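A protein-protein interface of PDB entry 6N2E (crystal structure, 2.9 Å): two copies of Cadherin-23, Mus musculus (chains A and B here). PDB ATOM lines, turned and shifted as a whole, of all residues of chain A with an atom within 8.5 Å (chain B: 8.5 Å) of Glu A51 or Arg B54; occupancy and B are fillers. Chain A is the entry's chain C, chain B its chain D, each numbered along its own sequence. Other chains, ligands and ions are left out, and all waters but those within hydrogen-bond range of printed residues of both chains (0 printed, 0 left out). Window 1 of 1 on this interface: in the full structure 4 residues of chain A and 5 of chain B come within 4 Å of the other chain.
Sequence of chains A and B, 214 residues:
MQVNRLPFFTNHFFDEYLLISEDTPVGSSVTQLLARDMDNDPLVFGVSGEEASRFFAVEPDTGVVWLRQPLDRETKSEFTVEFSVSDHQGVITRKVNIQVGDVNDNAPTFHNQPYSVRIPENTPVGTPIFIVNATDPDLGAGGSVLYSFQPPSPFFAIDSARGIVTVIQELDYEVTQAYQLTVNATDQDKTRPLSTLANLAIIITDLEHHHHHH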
ATOM      1  N   VAL A  47       7.136 -14.195  -8.741  1.00  0.00           N
ATOM      2  CA  VAL A  47       6.882 -15.331  -9.660  1.00  0.00           C
ATOM      3  C   VAL A  47       6.103 -14.821 -10.856  1.00  0.00           C
ATOM      4  O   VAL A  47       5.293 -13.895 -10.696  1.00  0.00           O
ATOM      5  CB  VAL A  47       6.116 -16.473  -8.971  1.00  0.00           C
ATOM      6  CG1 VAL A  47       4.694 -16.085  -8.598  1.00  0.00           C
ATOM      7  CG2 VAL A  47       6.112 -17.724  -9.831  1.00  0.00           C
ATOM      8  N   SER A  48       6.415 -15.394 -12.008  1.00  0.00           N
ATOM      9  CA  SER A  48       5.908 -14.994 -13.343  1.00  0.00           C
ATOM     10  C   SER A  48       5.255 -16.189 -14.025  1.00  0.00           C
ATOM     11  O   SER A  48       5.950 -17.219 -14.191  1.00  0.00           O
ATOM     12  CB  SER A  48       7.011 -14.459 -14.216  1.00  0.00           C
ATOM     13  OG  SER A  48       7.263 -13.088 -13.962  1.00  0.00           O
ATOM     14  N   GLY A  49       4.012 -16.004 -14.443  1.00  0.00           N
ATOM     15  CA  GLY A  49       3.242 -17.018 -15.174  1.00  0.00           C
ATOM     16  C   GLY A  49       1.925 -17.372 -14.497  1.00  0.00           C
ATOM     17  O   GLY A  49       1.934 -17.581 -13.258  1.00  0.00           O
ATOM     18  N   GLU A  50       0.884 -17.582 -15.321  1.00  0.00           N
ATOM     19  CA  GLU A  50      -0.457 -18.134 -14.974  1.00  0.00           C
ATOM     20  C   GLU A  50      -0.282 -19.413 -14.140  1.00  0.00           C
ATOM     21  O   GLU A  50      -0.845 -19.492 -13.026  1.00  0.00           O
ATOM     22  CB  GLU A  50      -1.221 -18.399 -16.281  1.00  0.00           C
ATOM     23  CG  GLU A  50      -2.496 -19.240 -16.157  1.00  0.00           C
ATOM     24  CD  GLU A  50      -3.589 -18.581 -15.348  1.00  0.00           C
ATOM     25  OE1 GLU A  50      -3.544 -17.344 -15.279  1.00  0.00           O
ATOM     26  OE2 GLU A  50      -4.448 -19.308 -14.761  1.00  0.00           O
ATOM     27  N   GLU A  51       0.382 -20.425 -14.700  1.00  0.00           N
ATOM     28  CA  GLU A  51       0.391 -21.791 -14.122  1.00  0.00           C
ATOM     29  C   GLU A  51       1.347 -21.830 -12.936  1.00  0.00           C
ATOM     30  O   GLU A  51       0.981 -22.408 -11.892  1.00  0.00           O
ATOM     31  CB  GLU A  51       0.735 -22.798 -15.216  1.00  0.00           C
ATOM     32  CG  GLU A  51      -0.427 -23.064 -16.148  1.00  0.00           C
ATOM     33  CD  GLU A  51      -0.274 -24.404 -16.831  1.00  0.00           C
ATOM     34  OE1 GLU A  51       0.903 -24.781 -17.079  1.00  0.00           O
ATOM     35  OE2 GLU A  51      -1.314 -25.090 -17.050  1.00  0.00           O
ATOM     36  N   ALA A  52       2.467 -21.131 -13.071  1.00  0.00           N
ATOM     37  CA  ALA A  52       3.544 -21.097 -12.068  1.00  0.00           C
ATOM     38  C   ALA A  52       3.001 -20.478 -10.788  1.00  0.00           C
ATOM     39  O   ALA A  52       3.428 -20.908  -9.725  1.00  0.00           O
ATOM     40  CB  ALA A  52       4.726 -20.331 -12.622  1.00  0.00           C
ATOM     41  N   SER A  53       2.239 -19.399 -10.956  1.00  0.00           N
ATOM     42  CA  SER A  53       1.740 -18.570  -9.845  1.00  0.00           C
ATOM     43  C   SER A  53       0.949 -19.431  -8.875  1.00  0.00           C
ATOM     44  O   SER A  53       1.152 -19.281  -7.659  1.00  0.00           O
ATOM     45  CB  SER A  53       0.903 -17.440 -10.350  1.00  0.00           C
ATOM     46  OG  SER A  53       0.335 -16.720  -9.271  1.00  0.00           O
ATOM     47  N   ARG A  54       0.109 -20.310  -9.423  1.00  0.00           N
ATOM     48  CA  ARG A  54      -0.731 -21.218  -8.629  1.00  0.00           C
ATOM     49  C   ARG A  54       0.134 -22.147  -7.789  1.00  0.00           C
ATOM     50  O   ARG A  54      -0.219 -22.377  -6.628  1.00  0.00           O
ATOM     51  CB  ARG A  54      -1.619 -22.072  -9.538  1.00  0.00           C
ATOM     52  CG  ARG A  54      -2.703 -21.288 -10.260  1.00  0.00           C
ATOM     53  CD  ARG A  54      -3.666 -22.184 -11.014  1.00  0.00           C
ATOM     54  NE  ARG A  54      -4.754 -21.385 -11.565  1.00  0.00           N
ATOM     55  CZ  ARG A  54      -5.836 -21.882 -12.154  1.00  0.00           C
ATOM     56  NH1 ARG A  54      -6.759 -21.060 -12.630  1.00  0.00           N
ATOM     57  NH2 ARG A  54      -5.976 -23.193 -12.285  1.00  0.00           N
ATOM     58  N   PHE A  55       1.184 -22.703  -8.385  1.00  0.00           N
ATOM     59  CA  PHE A  55       1.963 -23.774  -7.751  1.00  0.00           C
ATOM     60  C   PHE A  55       2.817 -23.200  -6.639  1.00  0.00           C
ATOM     61  O   PHE A  55       3.009 -23.915  -5.656  1.00  0.00           O
ATOM     62  CB  PHE A  55       2.819 -24.515  -8.771  1.00  0.00           C
ATOM     63  CG  PHE A  55       2.116 -25.701  -9.369  1.00  0.00           C
ATOM     64  CD1 PHE A  55       1.692 -26.750  -8.569  1.00  0.00           C
ATOM     65  CD2 PHE A  55       1.888 -25.775 -10.734  1.00  0.00           C
ATOM     66  CE1 PHE A  55       1.045 -27.842  -9.124  1.00  0.00           C
ATOM     67  CE2 PHE A  55       1.269 -26.883 -11.292  1.00  0.00           C
ATOM     68  CZ  PHE A  55       0.835 -27.906 -10.484  1.00  0.00           C
ATOM     69  N   PHE A  56       3.348 -22.002  -6.840  1.00  0.00           N
ATOM     70  CA  PHE A  56       4.392 -21.428  -5.972  1.00  0.00           C
ATOM     71  C   PHE A  56       4.029 -19.999  -5.580  1.00  0.00           C
ATOM     72  O   PHE A  56       3.522 -19.162  -6.387  1.00  0.00           O
ATOM     73  CB  PHE A  56       5.763 -21.487  -6.644  1.00  0.00           C
ATOM     74  CG  PHE A  56       6.142 -22.861  -7.128  1.00  0.00           C
ATOM     75  CD1 PHE A  56       6.542 -23.847  -6.238  1.00  0.00           C
ATOM     76  CD2 PHE A  56       6.088 -23.169  -8.479  1.00  0.00           C
ATOM     77  CE1 PHE A  56       6.882 -25.114  -6.692  1.00  0.00           C
ATOM     78  CE2 PHE A  56       6.444 -24.430  -8.936  1.00  0.00           C
ATOM     79  CZ  PHE A  56       6.829 -25.404  -8.042  1.00  0.00           C
ATOM     80  N   ARG A  68       2.156 -24.385  -3.151  1.00  0.00           N
ATOM     81  CA  ARG A  68       0.735 -24.018  -2.975  1.00  0.00           C
ATOM     82  C   ARG A  68      -0.150 -25.184  -3.421  1.00  0.00           C
ATOM     83  O   ARG A  68      -1.256 -25.310  -2.905  1.00  0.00           O
ATOM     84  CB  ARG A  68       0.399 -22.752  -3.770  1.00  0.00           C
ATOM     85  CG  ARG A  68       0.920 -21.467  -3.139  1.00  0.00           C
ATOM     86  CD  ARG A  68       0.609 -20.284  -4.029  1.00  0.00           C
ATOM     87  NE  ARG A  68      -0.707 -19.748  -3.779  1.00  0.00           N
ATOM     88  CZ  ARG A  68      -1.300 -18.839  -4.545  1.00  0.00           C
ATOM     89  NH1 ARG A  68      -2.490 -18.363  -4.205  1.00  0.00           N
ATOM     90  NH2 ARG A  68      -0.715 -18.434  -5.661  1.00  0.00           N
ATOM     91  N   GLN A  69       0.319 -26.017  -4.337  1.00  0.00           N
ATOM     92  CA  GLN A  69      -0.544 -27.074  -4.913  1.00  0.00           C
ATOM     93  C   GLN A  69       0.162 -28.428  -4.865  1.00  0.00           C
ATOM     94  O   GLN A  69       1.375 -28.502  -5.074  1.00  0.00           O
ATOM     95  CB  GLN A  69      -0.899 -26.680  -6.340  1.00  0.00           C
ATOM     96  CG  GLN A  69      -2.341 -26.252  -6.527  1.00  0.00           C
ATOM     97  CD  GLN A  69      -2.827 -26.709  -7.883  1.00  0.00           C
ATOM     98  OE1 GLN A  69      -3.071 -27.892  -8.109  1.00  0.00           O
ATOM     99  NE2 GLN A  69      -2.900 -25.783  -8.824  1.00  0.00           N
ATOM    100  N   THR A  75       1.608 -37.204 -13.177  1.00  0.00           N
ATOM    101  CA  THR A  75       0.867 -36.214 -13.999  1.00  0.00           C
ATOM    102  C   THR A  75       1.855 -35.380 -14.819  1.00  0.00           C
ATOM    103  O   THR A  75       1.819 -35.478 -16.061  1.00  0.00           O
ATOM    104  CB  THR A  75       0.017 -35.283 -13.127  1.00  0.00           C
ATOM    105  OG1 THR A  75      -0.989 -36.062 -12.480  1.00  0.00           O
ATOM    106  CG2 THR A  75      -0.620 -34.172 -13.933  1.00  0.00           C
ATOM    107  N   LYS A  76       2.613 -34.507 -14.149  1.00  0.00           N
ATOM    108  CA  LYS A  76       3.684 -33.692 -14.773  1.00  0.00           C
ATOM    109  C   LYS A  76       4.967 -33.876 -13.957  1.00  0.00           C
ATOM    110  O   LYS A  76       4.971 -33.548 -12.759  1.00  0.00           O
ATOM    111  CB  LYS A  76       3.254 -32.228 -14.893  1.00  0.00           C
ATOM    112  CG  LYS A  76       3.081 -31.731 -16.327  1.00  0.00           C
ATOM    113  CD  LYS A  76       3.336 -30.241 -16.505  1.00  0.00           C
ATOM    114  CE  LYS A  76       2.640 -29.388 -15.463  1.00  0.00           C
ATOM    115  NZ  LYS A  76       3.101 -27.984 -15.521  1.00  0.00           N
ATOM    116  N   PHE A  79       8.608 -28.892 -14.964  1.00  0.00           N
ATOM    117  CA  PHE A  79       8.142 -27.648 -15.610  1.00  0.00           C
ATOM    118  C   PHE A  79       9.080 -26.473 -15.365  1.00  0.00           C
ATOM    119  O   PHE A  79       9.884 -26.443 -14.401  1.00  0.00           O
ATOM    120  CB  PHE A  79       6.759 -27.299 -15.085  1.00  0.00           C
ATOM    121  CG  PHE A  79       6.629 -27.477 -13.599  1.00  0.00           C
ATOM    122  CD1 PHE A  79       7.138 -26.518 -12.748  1.00  0.00           C
ATOM    123  CD2 PHE A  79       6.010 -28.593 -13.051  1.00  0.00           C
ATOM    124  CE1 PHE A  79       6.991 -26.641 -11.375  1.00  0.00           C
ATOM    125  CE2 PHE A  79       5.886 -28.732 -11.676  1.00  0.00           C
ATOM    126  CZ  PHE A  79       6.349 -27.740 -10.839  1.00  0.00           C
ATOM    127  N   THR A  80       8.937 -25.479 -16.236  1.00  0.00           N
ATOM    128  CA  THR A  80       9.697 -24.215 -16.186  1.00  0.00           C
ATOM    129  C   THR A  80       8.894 -23.167 -15.448  1.00  0.00           C
ATOM    130  O   THR A  80       7.745 -22.896 -15.825  1.00  0.00           O
ATOM    131  CB  THR A  80      10.044 -23.672 -17.568  1.00  0.00           C
ATOM    132  OG1 THR A  80      10.801 -24.678 -18.221  1.00  0.00           O
ATOM    133  CG2 THR A  80      10.877 -22.414 -17.525  1.00  0.00           C
ATOM    134  N   VAL A  81       9.577 -22.512 -14.523  1.00  0.00           N
ATOM    135  CA  VAL A  81       9.038 -21.411 -13.688  1.00  0.00           C
ATOM    136  C   VAL A  81       9.993 -20.222 -13.779  1.00  0.00           C
ATOM    137  O   VAL A  81      11.216 -20.367 -13.531  1.00  0.00           O
ATOM    138  CB  VAL A  81       8.821 -21.874 -12.232  1.00  0.00           C
ATOM    139  CG1 VAL A  81       8.619 -20.703 -11.280  1.00  0.00           C
ATOM    140  CG2 VAL A  81       7.663 -22.856 -12.123  1.00  0.00           C
ATOM    141  N   VAL B  47      -7.865 -15.151 -27.649  1.00  0.00           N
ATOM    142  CA  VAL B  47      -8.058 -15.504 -26.217  1.00  0.00           C
ATOM    143  C   VAL B  47      -6.782 -15.181 -25.446  1.00  0.00           C
ATOM    144  O   VAL B  47      -5.720 -15.072 -26.057  1.00  0.00           O
ATOM    145  CB  VAL B  47      -8.491 -16.976 -26.061  1.00  0.00           C
ATOM    146  CG1 VAL B  47      -7.683 -17.912 -26.952  1.00  0.00           C
ATOM    147  CG2 VAL B  47      -8.442 -17.437 -24.608  1.00  0.00           C
ATOM    148  N   SER B  48      -6.932 -14.864 -24.171  1.00  0.00           N
ATOM    149  CA  SER B  48      -5.793 -14.552 -23.286  1.00  0.00           C
ATOM    150  C   SER B  48      -5.867 -15.375 -22.007  1.00  0.00           C
ATOM    151  O   SER B  48      -6.951 -15.903 -21.662  1.00  0.00           O
ATOM    152  CB  SER B  48      -5.745 -13.094 -22.985  1.00  0.00           C
ATOM    153  OG  SER B  48      -6.877 -12.714 -22.237  1.00  0.00           O
ATOM    154  N   GLY B  49      -4.747 -15.444 -21.294  1.00  0.00           N
ATOM    155  CA  GLY B  49      -4.546 -16.395 -20.188  1.00  0.00           C
ATOM    156  C   GLY B  49      -3.858 -17.688 -20.620  1.00  0.00           C
ATOM    157  O   GLY B  49      -4.145 -18.206 -21.724  1.00  0.00           O
ATOM    158  N   GLU B  50      -3.032 -18.275 -19.756  1.00  0.00           N
ATOM    159  CA  GLU B  50      -2.198 -19.441 -20.150  1.00  0.00           C
ATOM    160  C   GLU B  50      -3.106 -20.671 -20.261  1.00  0.00           C
ATOM    161  O   GLU B  50      -2.984 -21.427 -21.235  1.00  0.00           O
ATOM    162  CB  GLU B  50      -1.038 -19.609 -19.168  1.00  0.00           C
ATOM    163  CG  GLU B  50       0.081 -20.515 -19.667  1.00  0.00           C
ATOM    164  CD  GLU B  50       1.352 -20.484 -18.831  1.00  0.00           C
ATOM    165  OE1 GLU B  50       2.086 -19.487 -18.966  1.00  0.00           O
ATOM    166  OE2 GLU B  50       1.609 -21.459 -18.060  1.00  0.00           O
ATOM    167  N   GLU B  51      -3.971 -20.875 -19.284  1.00  0.00           N
ATOM    168  CA  GLU B  51      -4.776 -22.108 -19.275  1.00  0.00           C
ATOM    169  C   GLU B  51      -5.826 -22.022 -20.382  1.00  0.00           C
ATOM    170  O   GLU B  51      -6.010 -23.014 -21.121  1.00  0.00           O
ATOM    171  CB  GLU B  51      -5.299 -22.366 -17.863  1.00  0.00           C
ATOM    172  CG  GLU B  51      -4.143 -22.765 -16.948  1.00  0.00           C
ATOM    173  CD  GLU B  51      -4.313 -22.594 -15.448  1.00  0.00           C
ATOM    174  OE1 GLU B  51      -5.284 -23.198 -14.893  1.00  0.00           O
ATOM    175  OE2 GLU B  51      -3.418 -21.934 -14.826  1.00  0.00           O
ATOM    176  N   ALA B  52      -6.467 -20.866 -20.480  1.00  0.00           N
ATOM    177  CA  ALA B  52      -7.531 -20.650 -21.474  1.00  0.00           C
ATOM    178  C   ALA B  52      -6.958 -20.860 -22.867  1.00  0.00           C
ATOM    179  O   ALA B  52      -7.648 -21.475 -23.694  1.00  0.00           O
ATOM    180  CB  ALA B  52      -8.148 -19.276 -21.334  1.00  0.00           C
ATOM    181  N   SER B  53      -5.788 -20.266 -23.099  1.00  0.00           N
ATOM    182  CA  SER B  53      -5.064 -20.290 -24.380  1.00  0.00           C
ATOM    183  C   SER B  53      -4.765 -21.717 -24.789  1.00  0.00           C
ATOM    184  O   SER B  53      -4.687 -21.934 -25.982  1.00  0.00           O
ATOM    185  CB  SER B  53      -3.790 -19.479 -24.320  1.00  0.00           C
ATOM    186  OG  SER B  53      -4.077 -18.102 -24.155  1.00  0.00           O
ATOM    187  N   ARG B  54      -4.473 -22.574 -23.819  1.00  0.00           N
ATOM    188  CA  ARG B  54      -4.183 -24.006 -23.994  1.00  0.00           C
ATOM    189  C   ARG B  54      -5.442 -24.769 -24.376  1.00  0.00           C
ATOM    190  O   ARG B  54      -5.335 -25.635 -25.253  1.00  0.00           O
ATOM    191  CB  ARG B  54      -3.619 -24.524 -22.674  1.00  0.00           C
ATOM    192  CG  ARG B  54      -3.259 -25.993 -22.671  1.00  0.00           C
ATOM    193  CD  ARG B  54      -2.698 -26.340 -21.313  1.00  0.00           C
ATOM    194  NE  ARG B  54      -2.379 -27.748 -21.237  1.00  0.00           N
ATOM    195  CZ  ARG B  54      -1.690 -28.297 -20.252  1.00  0.00           C
ATOM    196  NH1 ARG B  54      -1.276 -27.544 -19.247  1.00  0.00           N
ATOM    197  NH2 ARG B  54      -1.419 -29.593 -20.269  1.00  0.00           N
ATOM    198  N   PHE B  55      -6.582 -24.450 -23.781  1.00  0.00           N
ATOM    199  CA  PHE B  55      -7.841 -25.181 -24.007  1.00  0.00           C
ATOM    200  C   PHE B  55      -8.536 -24.717 -25.281  1.00  0.00           C
ATOM    201  O   PHE B  55      -9.233 -25.535 -25.875  1.00  0.00           O
ATOM    202  CB  PHE B  55      -8.794 -25.035 -22.820  1.00  0.00           C
ATOM    203  CG  PHE B  55      -8.598 -26.088 -21.761  1.00  0.00           C
ATOM    204  CD1 PHE B  55      -7.590 -25.969 -20.815  1.00  0.00           C
ATOM    205  CD2 PHE B  55      -9.391 -27.220 -21.742  1.00  0.00           C
ATOM    206  CE1 PHE B  55      -7.401 -26.948 -19.855  1.00  0.00           C
ATOM    207  CE2 PHE B  55      -9.196 -28.199 -20.783  1.00  0.00           C
ATOM    208  CZ  PHE B  55      -8.203 -28.060 -19.843  1.00  0.00           C
ATOM    209  N   PHE B  56      -8.385 -23.447 -25.626  1.00  0.00           N
ATOM    210  CA  PHE B  56      -9.182 -22.794 -26.673  1.00  0.00           C
ATOM    211  C   PHE B  56      -8.276 -22.005 -27.605  1.00  0.00           C
ATOM    212  O   PHE B  56      -7.324 -21.280 -27.180  1.00  0.00           O
ATOM    213  CB  PHE B  56     -10.252 -21.893 -26.060  1.00  0.00           C
ATOM    214  CG  PHE B  56     -11.241 -22.597 -25.168  1.00  0.00           C
ATOM    215  CD1 PHE B  56     -12.318 -23.280 -25.713  1.00  0.00           C
ATOM    216  CD2 PHE B  56     -11.123 -22.533 -23.789  1.00  0.00           C
ATOM    217  CE1 PHE B  56     -13.279 -23.857 -24.895  1.00  0.00           C
ATOM    218  CE2 PHE B  56     -12.068 -23.138 -22.973  1.00  0.00           C
ATOM    219  CZ  PHE B  56     -13.148 -23.794 -23.527  1.00  0.00           C
ATOM    220  N   ALA B  57      -8.685 -22.039 -28.872  1.00  0.00           N
ATOM    221  CA  ALA B  57      -8.090 -21.316 -30.012  1.00  0.00           C
ATOM    222  C   ALA B  57      -9.164 -20.480 -30.694  1.00  0.00           C
ATOM    223  O   ALA B  57     -10.351 -20.849 -30.648  1.00  0.00           O
ATOM    224  CB  ALA B  57      -7.481 -22.285 -30.996  1.00  0.00           C
ATOM    225  N   TRP B  66     -12.378 -22.658 -31.208  1.00  0.00           N
ATOM    226  CA  TRP B  66     -11.884 -24.032 -31.447  1.00  0.00           C
ATOM    227  C   TRP B  66     -11.486 -24.674 -30.113  1.00  0.00           C
ATOM    228  O   TRP B  66     -10.748 -24.047 -29.296  1.00  0.00           O
ATOM    229  CB  TRP B  66     -10.671 -24.017 -32.391  1.00  0.00           C
ATOM    230  CG  TRP B  66     -10.973 -24.140 -33.855  1.00  0.00           C
ATOM    231  CD1 TRP B  66     -11.949 -23.487 -34.555  1.00  0.00           C
ATOM    232  CD2 TRP B  66     -10.224 -24.896 -34.827  1.00  0.00           C
ATOM    233  NE1 TRP B  66     -11.871 -23.794 -35.890  1.00  0.00           N
ATOM    234  CE2 TRP B  66     -10.822 -24.656 -36.087  1.00  0.00           C
ATOM    235  CE3 TRP B  66      -9.114 -25.749 -34.759  1.00  0.00           C
ATOM    236  CZ2 TRP B  66     -10.353 -25.257 -37.258  1.00  0.00           C
ATOM    237  CZ3 TRP B  66      -8.641 -26.322 -35.921  1.00  0.00           C
ATOM    238  CH2 TRP B  66      -9.256 -26.082 -37.152  1.00  0.00           C
ATOM    239  N   LEU B  67     -11.997 -25.868 -29.873  1.00  0.00           N
ATOM    240  CA  LEU B  67     -11.530 -26.679 -28.726  1.00  0.00           C
ATOM    241  C   LEU B  67     -10.164 -27.272 -29.056  1.00  0.00           C
ATOM    242  O   LEU B  67     -10.029 -27.971 -30.069  1.00  0.00           O
ATOM    243  CB  LEU B  67     -12.541 -27.784 -28.419  1.00  0.00           C
ATOM    244  CG  LEU B  67     -12.347 -28.437 -27.057  1.00  0.00           C
ATOM    245  CD1 LEU B  67     -12.439 -27.392 -25.952  1.00  0.00           C
ATOM    246  CD2 LEU B  67     -13.359 -29.549 -26.854  1.00  0.00           C
ATOM    247  N   ARG B  68      -9.179 -27.043 -28.206  1.00  0.00           N
ATOM    248  CA  ARG B  68      -7.844 -27.613 -28.447  1.00  0.00           C
ATOM    249  C   ARG B  68      -7.743 -28.956 -27.740  1.00  0.00           C
ATOM    250  O   ARG B  68      -7.097 -29.869 -28.280  1.00  0.00           O
ATOM    251  CB  ARG B  68      -6.771 -26.642 -27.978  1.00  0.00           C
ATOM    252  CG  ARG B  68      -6.468 -25.597 -29.033  1.00  0.00           C
ATOM    253  CD  ARG B  68      -5.177 -24.853 -28.814  1.00  0.00           C
ATOM    254  NE  ARG B  68      -4.009 -25.695 -28.662  1.00  0.00           N
ATOM    255  CZ  ARG B  68      -2.761 -25.245 -28.698  1.00  0.00           C
ATOM    256  NH1 ARG B  68      -2.526 -23.956 -28.885  1.00  0.00           N
ATOM    257  NH2 ARG B  68      -1.752 -26.084 -28.537  1.00  0.00           N
ATOM    258  N   GLN B  69      -8.301 -29.057 -26.543  1.00  0.00           N
ATOM    259  CA  GLN B  69      -8.153 -30.282 -25.725  1.00  0.00           C
ATOM    260  C   GLN B  69      -9.497 -30.626 -25.111  1.00  0.00           C
ATOM    261  O   GLN B  69     -10.338 -29.746 -24.929  1.00  0.00           O
ATOM    262  CB  GLN B  69      -7.069 -30.059 -24.678  1.00  0.00           C
ATOM    263  CG  GLN B  69      -5.701 -29.794 -25.293  1.00  0.00           C
ATOM    264  CD  GLN B  69      -4.633 -29.607 -24.242  1.00  0.00           C
ATOM    265  OE1 GLN B  69      -4.893 -29.069 -23.163  1.00  0.00           O
ATOM    266  NE2 GLN B  69      -3.418 -30.051 -24.551  1.00  0.00           N
ATOM    267  N   PRO B  70      -9.735 -31.913 -24.775  1.00  0.00           N
ATOM    268  CA  PRO B  70     -11.050 -32.353 -24.309  1.00  0.00           C
ATOM    269  C   PRO B  70     -11.349 -31.810 -22.903  1.00  0.00           C
ATOM    270  O   PRO B  70     -10.429 -31.725 -22.092  1.00  0.00           O
ATOM    271  CB  PRO B  70     -10.931 -33.879 -24.332  1.00  0.00           C
ATOM    272  CG  PRO B  70      -9.462 -34.126 -24.071  1.00  0.00           C
ATOM    273  CD  PRO B  70      -8.740 -32.994 -24.771  1.00  0.00           C
ATOM    274  N   LYS B  76     -13.207 -30.315 -13.664  1.00  0.00           N
ATOM    275  CA  LYS B  76     -13.662 -28.901 -13.622  1.00  0.00           C
ATOM    276  C   LYS B  76     -14.972 -28.802 -14.382  1.00  0.00           C
ATOM    277  O   LYS B  76     -15.032 -29.290 -15.514  1.00  0.00           O
ATOM    278  CB  LYS B  76     -12.622 -27.963 -14.242  1.00  0.00           C
ATOM    279  CG  LYS B  76     -11.386 -27.743 -13.381  1.00  0.00           C
ATOM    280  CD  LYS B  76     -10.409 -26.734 -13.969  1.00  0.00           C
ATOM    281  CE  LYS B  76      -8.988 -26.955 -13.481  1.00  0.00           C
ATOM    282  NZ  LYS B  76      -8.142 -25.763 -13.706  1.00  0.00           N
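OE2 of Glu A51 is in salt-bridge range of NH1 of Arg B54 (3.3 Å). OE2 of Glu A50 lies close to OE2 of Glu B51 (2.8 Å). NH2 of Arg A54 is in salt-bridge range of OE1 of Glu B51 (2.7 Å).
Glu B50 touches its own counterpart, Glu A50. Glu A50 touches Glu B51, and with the chains exchanged Glu A51 touches Glu B50. Glu A51 touches Arg B54, and with the chains exchanged Arg A54 touches Glu B51. Arg A54 touches Lys B76, but with the chains exchanged Lys A76 does not touch Arg B54 (5.7 Å). Of the 7 pairs that touch across the chains among the printed residues, 6 have their exchanged pair printed and touching as well.
CB of Glu B50 touches CB of Glu A50, 3.1 Å away. OE2 of Glu B50 touches CG of Glu A51, at 3.2 Å. Glu B51 touches Glu A51 (OE2 to CG, 3.5 Å). NZ of Lys B76 touches NH2 of Arg A54, 3.6 Å away.
Glu A51 touches just these residues of chain B: Glu B50, Glu B51 and Arg B54. Arg B54 touches one residue of chain A. No residue of chain B comes within 4 Å of Ala A52. Printed residues of chain A within 4 Å of Glu B50: Glu A50 and Glu A51. Of the printed residues of chain B, Glu A50 touches Glu B50 and Glu B51. Of the printed residues of chain A, Glu B51 touches Glu A50 (2.8 Å), Glu A51 (3.5 Å) and Arg A54 (2.7 Å). The nearest residue of chain A that does not touch Arg B54 is Lys A76 (5.7 Å).
NE of Arg B54 lies within hydrogen-bond range of OE1 of Gln B69. OE2 of Glu A50 lies within salt-bridge range of NH1 of Arg A54, 3.6 Å away.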
